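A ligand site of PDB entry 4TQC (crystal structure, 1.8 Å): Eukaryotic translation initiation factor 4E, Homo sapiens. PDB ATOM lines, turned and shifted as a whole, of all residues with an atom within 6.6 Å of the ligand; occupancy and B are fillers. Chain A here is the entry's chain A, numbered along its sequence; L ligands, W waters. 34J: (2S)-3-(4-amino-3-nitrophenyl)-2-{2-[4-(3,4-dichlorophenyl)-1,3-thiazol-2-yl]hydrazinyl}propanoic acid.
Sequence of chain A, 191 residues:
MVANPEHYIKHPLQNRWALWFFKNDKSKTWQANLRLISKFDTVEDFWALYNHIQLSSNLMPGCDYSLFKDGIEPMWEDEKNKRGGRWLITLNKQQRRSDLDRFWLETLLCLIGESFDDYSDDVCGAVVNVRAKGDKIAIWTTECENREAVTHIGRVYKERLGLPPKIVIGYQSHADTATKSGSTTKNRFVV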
ATOM      1  N   LEU A  19     -16.436 -11.270  30.498  1.00  0.00           N
ATOM      2  CA  LEU A  19     -15.374 -11.338  29.497  1.00  0.00           C
ATOM      3  C   LEU A  19     -15.937 -11.038  28.105  1.00  0.00           C
ATOM      4  O   LEU A  19     -16.907 -11.662  27.687  1.00  0.00           O
ATOM      5  CB  LEU A  19     -14.721 -12.720  29.499  1.00  0.00           C
ATOM      6  CG  LEU A  19     -13.732 -13.019  28.374  1.00  0.00           C
ATOM      7  CD1 LEU A  19     -12.540 -12.090  28.446  1.00  0.00           C
ATOM      8  CD2 LEU A  19     -13.274 -14.469  28.413  1.00  0.00           C
ATOM      9  N   PHE A  21     -15.020 -10.455  23.839  1.00  0.00           N
ATOM     10  CA  PHE A  21     -14.111 -10.554  22.697  1.00  0.00           C
ATOM     11  C   PHE A  21     -14.407  -9.458  21.689  1.00  0.00           C
ATOM     12  O   PHE A  21     -15.542  -9.009  21.561  1.00  0.00           O
ATOM     13  CB  PHE A  21     -14.220 -11.908  21.988  1.00  0.00           C
ATOM     14  CG  PHE A  21     -13.595 -13.058  22.726  1.00  0.00           C
ATOM     15  CD1 PHE A  21     -13.083 -12.899  24.001  1.00  0.00           C
ATOM     16  CD2 PHE A  21     -13.511 -14.294  22.120  1.00  0.00           C
ATOM     17  CE1 PHE A  21     -12.508 -13.971  24.660  1.00  0.00           C
ATOM     18  CE2 PHE A  21     -12.932 -15.366  22.771  1.00  0.00           C
ATOM     19  CZ  PHE A  21     -12.432 -15.201  24.052  1.00  0.00           C
ATOM     20  N   PHE A  22     -13.376  -9.062  20.950  1.00  0.00           N
ATOM     21  CA  PHE A  22     -13.524  -8.183  19.802  1.00  0.00           C
ATOM     22  C   PHE A  22     -12.718  -8.765  18.658  1.00  0.00           C
ATOM     23  O   PHE A  22     -11.530  -9.025  18.804  1.00  0.00           O
ATOM     24  CB  PHE A  22     -13.060  -6.766  20.140  1.00  0.00           C
ATOM     25  CG  PHE A  22     -13.146  -5.805  18.996  1.00  0.00           C
ATOM     26  CD1 PHE A  22     -14.193  -4.900  18.909  1.00  0.00           C
ATOM     27  CD2 PHE A  22     -12.184  -5.794  17.994  1.00  0.00           C
ATOM     28  CE1 PHE A  22     -14.273  -4.012  17.855  1.00  0.00           C
ATOM     29  CE2 PHE A  22     -12.271  -4.914  16.939  1.00  0.00           C
ATOM     30  CZ  PHE A  22     -13.307  -4.022  16.867  1.00  0.00           C
ATOM     31  N   LYS A  23     -13.373  -8.976  17.529  1.00  0.00           N
ATOM     32  CA  LYS A  23     -12.710  -9.464  16.321  1.00  0.00           C
ATOM     33  C   LYS A  23     -12.585  -8.325  15.330  1.00  0.00           C
ATOM     34  O   LYS A  23     -13.601  -7.784  14.871  1.00  0.00           O
ATOM     35  CB  LYS A  23     -13.485 -10.624  15.703  1.00  0.00           C
ATOM     36  CG  LYS A  23     -12.872 -11.211  14.432  1.00  0.00           C
ATOM     37  CD  LYS A  23     -13.904 -11.958  13.608  1.00  0.00           C
ATOM     38  CE  LYS A  23     -13.279 -12.703  12.432  1.00  0.00           C
ATOM     39  NZ  LYS A  23     -12.608 -11.780  11.473  1.00  0.00           N
ATOM     40  N   ASN A  24     -11.363  -7.954  14.979  1.00  0.00           N
ATOM     41  CA  ASN A  24     -11.157  -6.886  14.013  1.00  0.00           C
ATOM     42  C   ASN A  24     -11.853  -7.201  12.695  1.00  0.00           C
ATOM     43  O   ASN A  24     -11.680  -8.274  12.136  1.00  0.00           O
ATOM     44  CB  ASN A  24      -9.664  -6.641  13.760  1.00  0.00           C
ATOM     45  CG  ASN A  24      -9.423  -5.395  12.926  1.00  0.00           C
ATOM     46  OD1 ASN A  24     -10.155  -4.418  13.028  1.00  0.00           O
ATOM     47  ND2 ASN A  24      -8.385  -5.435  12.100  1.00  0.00           N
ATOM     48  N   ASP A  25     -12.653  -6.249  12.224  1.00  0.00           N
ATOM     49  CA  ASP A  25     -13.310  -6.369  10.940  1.00  0.00           C
ATOM     50  C   ASP A  25     -13.674  -4.977  10.442  1.00  0.00           C
ATOM     51  O   ASP A  25     -14.702  -4.418  10.816  1.00  0.00           O
ATOM     52  CB  ASP A  25     -14.546  -7.264  11.034  1.00  0.00           C
ATOM     53  CG  ASP A  25     -14.993  -7.791   9.685  1.00  0.00           C
ATOM     54  OD1 ASP A  25     -14.633  -7.191   8.653  1.00  0.00           O
ATOM     55  OD2 ASP A  25     -15.716  -8.813   9.653  1.00  0.00           O
ATOM     56  N   LYS A  28     -17.086  -3.799   9.013  1.00  0.00           N
ATOM     57  CA  LYS A  28     -18.225  -3.621   9.902  1.00  0.00           C
ATOM     58  C   LYS A  28     -17.999  -2.453  10.861  1.00  0.00           C
ATOM     59  O   LYS A  28     -16.865  -2.133  11.213  1.00  0.00           O
ATOM     60  CB  LYS A  28     -18.489  -4.892  10.705  1.00  0.00           C
ATOM     61  CG  LYS A  28     -18.841  -6.105   9.867  1.00  0.00           C
ATOM     62  CD  LYS A  28     -19.557  -7.157  10.689  1.00  0.00           C
ATOM     63  CE  LYS A  28     -19.851  -8.408   9.866  1.00  0.00           C
ATOM     64  NZ  LYS A  28     -18.614  -9.177   9.554  1.00  0.00           N
ATOM     65  N   ALA A  32     -20.279  -3.733  16.142  1.00  0.00           N
ATOM     66  CA  ALA A  32     -20.764  -4.984  15.585  1.00  0.00           C
ATOM     67  C   ALA A  32     -19.782  -6.126  15.834  1.00  0.00           C
ATOM     68  O   ALA A  32     -20.149  -7.295  15.795  1.00  0.00           O
ATOM     69  CB  ALA A  32     -21.008  -4.837  14.094  1.00  0.00           C
ATOM     70  N   ASN A  33     -18.530  -5.773  16.117  1.00  0.00           N
ATOM     71  CA  ASN A  33     -17.465  -6.749  16.300  1.00  0.00           C
ATOM     72  C   ASN A  33     -17.295  -7.215  17.744  1.00  0.00           C
ATOM     73  O   ASN A  33     -16.446  -8.067  18.028  1.00  0.00           O
ATOM     74  CB  ASN A  33     -16.143  -6.173  15.803  1.00  0.00           C
ATOM     75  CG  ASN A  33     -16.157  -5.882  14.321  1.00  0.00           C
ATOM     76  OD1 ASN A  33     -16.764  -6.607  13.528  1.00  0.00           O
ATOM     77  ND2 ASN A  33     -15.488  -4.799  13.926  1.00  0.00           N
ATOM     78  N   LEU A  34     -18.084  -6.651  18.656  1.00  0.00           N
ATOM     79  CA  LEU A  34     -18.023  -7.020  20.062  1.00  0.00           C
ATOM     80  C   LEU A  34     -18.879  -8.233  20.380  1.00  0.00           C
ATOM     81  O   LEU A  34     -19.978  -8.389  19.843  1.00  0.00           O
ATOM     82  CB  LEU A  34     -18.477  -5.852  20.934  1.00  0.00           C
ATOM     83  CG  LEU A  34     -17.419  -4.916  21.515  1.00  0.00           C
ATOM     84  CD1 LEU A  34     -18.122  -3.841  22.303  1.00  0.00           C
ATOM     85  CD2 LEU A  34     -16.421  -5.630  22.394  1.00  0.00           C
ATOM     86  N   ARG A  35     -18.370  -9.086  21.257  1.00  0.00           N
ATOM     87  CA  ARG A  35     -19.076 -10.292  21.672  1.00  0.00           C
ATOM     88  C   ARG A  35     -18.925 -10.537  23.169  1.00  0.00           C
ATOM     89  O   ARG A  35     -17.812 -10.644  23.673  1.00  0.00           O
ATOM     90  CB  ARG A  35     -18.557 -11.514  20.895  1.00  0.00           C
ATOM     91  CG  ARG A  35     -18.796 -11.488  19.397  1.00  0.00           C
ATOM     92  CD  ARG A  35     -20.265 -11.597  19.048  1.00  0.00           C
ATOM     93  NE  ARG A  35     -20.459 -11.742  17.606  1.00  0.00           N
ATOM     94  CZ  ARG A  35     -20.464 -10.726  16.746  1.00  0.00           C
ATOM     95  NH1 ARG A  35     -20.295  -9.488  17.177  1.00  0.00           N
ATOM     96  NH2 ARG A  35     -20.645 -10.956  15.452  1.00  0.00           N
ATOM     97  N   ILE A  37     -18.787 -12.924  26.050  1.00  0.00           N
ATOM     98  CA  ILE A  37     -18.460 -14.346  26.119  1.00  0.00           C
ATOM     99  C   ILE A  37     -19.104 -15.028  27.324  1.00  0.00           C
ATOM    100  O   ILE A  37     -19.910 -15.927  27.156  1.00  0.00           O
ATOM    101  CB  ILE A  37     -16.942 -14.560  26.168  1.00  0.00           C
ATOM    102  CG1 ILE A  37     -16.265 -13.795  25.030  1.00  0.00           C
ATOM    103  CG2 ILE A  37     -16.607 -16.046  26.089  1.00  0.00           C
ATOM    104  CD1 ILE A  37     -16.819 -14.111  23.653  1.00  0.00           C
ATOM    105  N   SER A  38     -18.716 -14.618  28.530  1.00  0.00           N
ATOM    106  CA  SER A  38     -19.285 -15.210  29.722  1.00  0.00           C
ATOM    107  C   SER A  38     -19.071 -14.322  30.931  1.00  0.00           C
ATOM    108  O   SER A  38     -18.354 -13.312  30.851  1.00  0.00           O
ATOM    109  CB  SER A  38     -18.672 -16.589  29.979  1.00  0.00           C
ATOM    110  OG  SER A  38     -17.255 -16.536  29.979  1.00  0.00           O
ATOM    111  N   LEU A  49     -12.052 -20.114  33.749  1.00  0.00           N
ATOM    112  CA  LEU A  49     -12.114 -19.397  32.490  1.00  0.00           C
ATOM    113  C   LEU A  49     -10.710 -19.043  31.989  1.00  0.00           C
ATOM    114  O   LEU A  49     -10.381 -19.310  30.828  1.00  0.00           O
ATOM    115  CB  LEU A  49     -12.947 -18.120  32.640  1.00  0.00           C
ATOM    116  CG  LEU A  49     -13.165 -17.315  31.366  1.00  0.00           C
ATOM    117  CD1 LEU A  49     -13.871 -18.151  30.304  1.00  0.00           C
ATOM    118  CD2 LEU A  49     -13.954 -16.056  31.667  1.00  0.00           C
ATOM    119  N   HIS A  52      -8.763 -22.067  30.826  1.00  0.00           N
ATOM    120  CA  HIS A  52      -9.333 -22.652  29.632  1.00  0.00           C
ATOM    121  C   HIS A  52      -8.863 -21.899  28.383  1.00  0.00           C
ATOM    122  O   HIS A  52      -8.480 -22.509  27.383  1.00  0.00           O
ATOM    123  CB  HIS A  52     -10.857 -22.637  29.726  1.00  0.00           C
ATOM    124  CG  HIS A  52     -11.542 -23.055  28.458  1.00  0.00           C
ATOM    125  ND1 HIS A  52     -12.518 -22.291  27.859  1.00  0.00           N
ATOM    126  CD2 HIS A  52     -11.384 -24.153  27.685  1.00  0.00           C
ATOM    127  CE1 HIS A  52     -12.942 -22.904  26.762  1.00  0.00           C
ATOM    128  NE2 HIS A  52     -12.265 -24.028  26.638  1.00  0.00           N
ATOM    129  N   ILE A  53      -8.907 -20.572  28.448  1.00  0.00           N
ATOM    130  CA  ILE A  53      -8.484 -19.745  27.330  1.00  0.00           C
ATOM    131  C   ILE A  53      -6.985 -19.840  27.096  1.00  0.00           C
ATOM    132  O   ILE A  53      -6.534 -19.814  25.951  1.00  0.00           O
ATOM    133  CB  ILE A  53      -8.885 -18.271  27.566  1.00  0.00           C
ATOM    134  CG1 ILE A  53     -10.402 -18.132  27.421  1.00  0.00           C
ATOM    135  CG2 ILE A  53      -8.192 -17.342  26.573  1.00  0.00           C
ATOM    136  CD1 ILE A  53     -10.968 -16.839  27.970  1.00  0.00           C
ATOM    137  N   GLN A  54      -6.206 -19.956  28.164  1.00  0.00           N
ATOM    138  CA  GLN A  54      -4.753 -20.113  28.032  1.00  0.00           C
ATOM    139  C   GLN A  54      -4.426 -21.403  27.282  1.00  0.00           C
ATOM    140  O   GLN A  54      -3.471 -21.447  26.507  1.00  0.00           O
ATOM    141  CB  GLN A  54      -4.066 -20.108  29.396  1.00  0.00           C
ATOM    142  CG  GLN A  54      -4.016 -18.738  30.078  1.00  0.00           C
ATOM    143  CD  GLN A  54      -3.569 -17.624  29.150  1.00  0.00           C
ATOM    144  OE1 GLN A  54      -4.381 -16.835  28.687  1.00  0.00           O
ATOM    145  NE2 GLN A  54      -2.270 -17.563  28.882  1.00  0.00           N
ATOM    146  N   LEU A  55      -5.205 -22.445  27.531  1.00  0.00           N
ATOM    147  CA  LEU A  55      -5.030 -23.708  26.824  1.00  0.00           C
ATOM    148  C   LEU A  55      -5.712 -23.691  25.462  1.00  0.00           C
ATOM    149  O   LEU A  55      -5.407 -24.506  24.595  1.00  0.00           O
ATOM    150  CB  LEU A  55      -5.575 -24.875  27.667  1.00  0.00           C
ATOM    151  CG  LEU A  55      -4.929 -25.143  29.039  1.00  0.00           C
ATOM    152  CD1 LEU A  55      -5.653 -26.272  29.750  1.00  0.00           C
ATOM    153  CD2 LEU A  55      -3.443 -25.446  28.913  1.00  0.00           C
ATOM    154  N   SER A  56      -6.648 -22.755  25.291  1.00  0.00           N
ATOM    155  CA  SER A  56      -7.493 -22.733  24.109  1.00  0.00           C
ATOM    156  C   SER A  56      -7.364 -21.351  23.454  1.00  0.00           C
ATOM    157  O   SER A  56      -7.169 -21.232  22.239  1.00  0.00           O
ATOM    158  CB  SER A  56      -8.941 -23.068  24.493  1.00  0.00           C
ATOM    159  OG  SER A  56      -8.963 -24.268  25.257  1.00  0.00           O
ATOM    160  N   MET A  60      -5.553 -14.503  16.582  1.00  0.00           N
ATOM    161  CA  MET A  60      -5.564 -13.598  17.715  1.00  0.00           C
ATOM    162  C   MET A  60      -5.237 -12.131  17.372  1.00  0.00           C
ATOM    163  O   MET A  60      -5.668 -11.232  18.084  1.00  0.00           O
ATOM    164  CB  MET A  60      -4.585 -14.084  18.789  1.00  0.00           C
ATOM    165  CG  MET A  60      -4.712 -13.376  20.126  1.00  0.00           C
ATOM    166  SD  MET A  60      -6.351 -13.516  20.860  1.00  0.00           S
ATOM    167  CE  MET A  60      -6.452 -15.284  21.132  1.00  0.00           C
ATOM    168  N   ASP A  64      -9.352  -8.150  20.545  1.00  0.00           N
ATOM    169  CA  ASP A  64      -9.244  -7.680  21.923  1.00  0.00           C
ATOM    170  C   ASP A  64      -9.905  -8.650  22.886  1.00  0.00           C
ATOM    171  O   ASP A  64     -10.875  -9.336  22.535  1.00  0.00           O
ATOM    172  CB  ASP A  64      -9.886  -6.302  22.111  1.00  0.00           C
ATOM    173  CG  ASP A  64      -9.498  -5.305  21.040  1.00  0.00           C
ATOM    174  OD1 ASP A  64      -8.442  -5.484  20.398  1.00  0.00           O
ATOM    175  OD2 ASP A  64     -10.248  -4.328  20.861  1.00  0.00           O
ATOM    176  N   TYR A  65      -9.364  -8.705  24.101  1.00  0.00           N
ATOM    177  CA  TYR A  65     -10.047  -9.264  25.265  1.00  0.00           C
ATOM    178  C   TYR A  65     -10.380  -8.100  26.179  1.00  0.00           C
ATOM    179  O   TYR A  65      -9.554  -7.212  26.377  1.00  0.00           O
ATOM    180  CB  TYR A  65      -9.168 -10.246  26.044  1.00  0.00           C
ATOM    181  CG  TYR A  65      -8.915 -11.599  25.426  1.00  0.00           C
ATOM    182  CD1 TYR A  65      -9.748 -12.127  24.456  1.00  0.00           C
ATOM    183  CD2 TYR A  65      -7.824 -12.357  25.846  1.00  0.00           C
ATOM    184  CE1 TYR A  65      -9.491 -13.377  23.914  1.00  0.00           C
ATOM    185  CE2 TYR A  65      -7.571 -13.592  25.313  1.00  0.00           C
ATOM    186  CZ  TYR A  65      -8.405 -14.106  24.341  1.00  0.00           C
ATOM    187  OH  TYR A  65      -8.146 -15.349  23.812  1.00  0.00           O
HETATM  188  C10 34J L   1     -13.643 -17.796  18.185  1.00  0.00           C
HETATM  189  C13 34J L   1     -13.203 -18.756  21.562  1.00  0.00           C
HETATM  190  C15 34J L   1     -14.571 -18.577  23.539  1.00  0.00           C
HETATM  191  C20 34J L   1     -12.315 -19.563  22.265  1.00  0.00           C
HETATM  192  C21 34J L   1     -11.717 -18.437  19.746  1.00  0.00           C
HETATM  193  C26 34J L   1     -16.064 -14.145  16.638  1.00  0.00           C
HETATM  194 CL17 34J L   1     -13.982 -19.775  25.863  1.00  0.00          CL
HETATM  195 CL19 34J L   1     -11.463 -20.903  24.509  1.00  0.00          CL
HETATM  196  N01 34J L   1     -17.057 -10.543  16.361  1.00  0.00           N
HETATM  197  C02 34J L   1     -16.850 -11.942  16.040  1.00  0.00           C
HETATM  198  C03 34J L   1     -17.234 -12.424  14.805  1.00  0.00           C
HETATM  199  C04 34J L   1     -17.045 -13.754  14.475  1.00  0.00           C
HETATM  200  C05 34J L   1     -16.455 -14.621  15.400  1.00  0.00           C
HETATM  201  C06 34J L   1     -16.235 -16.106  15.031  1.00  0.00           C
HETATM  202  C07 34J L   1     -14.778 -16.583  14.863  1.00  0.00           C
HETATM  203  N08 34J L   1     -14.041 -16.994  15.929  1.00  0.00           N
HETATM  204  N09 34J L   1     -14.553 -17.386  17.055  1.00  0.00           N
HETATM  205  N11 34J L   1     -14.000 -18.094  19.453  1.00  0.00           N
HETATM  206  C12 34J L   1     -12.989 -18.439  20.298  1.00  0.00           C
HETATM  207  C14 34J L   1     -14.318 -18.268  22.205  1.00  0.00           C
HETATM  208  C16 34J L   1     -13.702 -19.379  24.234  1.00  0.00           C
HETATM  209  C18 34J L   1     -12.575 -19.865  23.596  1.00  0.00           C
HETATM  210  S22 34J L   1     -11.947 -17.977  18.103  1.00  0.00           S
HETATM  211  C23 34J L   1     -14.074 -16.148  13.623  1.00  0.00           C
HETATM  212  O24 34J L   1     -12.819 -16.202  13.533  1.00  0.00           O
HETATM  213  O25 34J L   1     -14.776 -15.704  12.614  1.00  0.00           O
HETATM  214  C27 34J L   1     -16.260 -12.809  16.964  1.00  0.00           C
HETATM  215  N28 34J L   1     -15.832 -12.313  18.294  1.00  0.00           N
HETATM  216  O29 34J L   1     -15.787 -11.049  18.541  1.00  0.00           O
HETATM  217  O30 34J L   1     -15.491 -13.148  19.198  1.00  0.00           O
HETATM  218  O   HOH W   1     -19.248 -12.574  12.120  1.00  0.00           O
HETATM  219  O   HOH W   2     -11.156 -18.072  15.723  1.00  0.00           O
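The backbone carbonyl oxygen (O) of Ala 32 lies within hydrogen-bond range of the guanidinium group (NH1) of Arg 35 (2.6 Å).
The backbone NH (N) of Lys 23 sits at hydrogen-bond distance from the backbone carbonyl oxygen (O) of Asn 33, at 3.2 Å.
ND2 of Asn 33 lies within hydrogen-bond range of O of Asp 25 (3.2 Å).
O of Arg 35 is in hydrogen-bond range of N of Phe 21 (2.8 Å).
O of Phe 22 lies within hydrogen-bond range of N of Asp 64, at 2.9 Å.
The side-chain hydroxyl of Ser 56 lies within hydrogen-bond range of the backbone carbonyl oxygen of His 52.
Merely in contact with the ligand: Arg 35 (3.2 Å), Phe 21 (3.3 Å), Ser 56 (3.3 Å), His 52 (3.4 Å) and Phe 22 (3.8 Å).
Hydrophobic or aromatic side chains that line the ligand: Phe 21 and His 52.
Of the 22 residues printed, 7 come within 4 Å of the ligand.
The backbone carbonyl oxygen (O) of Asn 33 is in hydrogen-bond range of a nitrogen (N01) of the ligand, at 3.0 Å.
The backbone NH of Lys 23 sits at hydrogen-bond distance from an oxygen (O29) of the ligand (3.3 Å).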
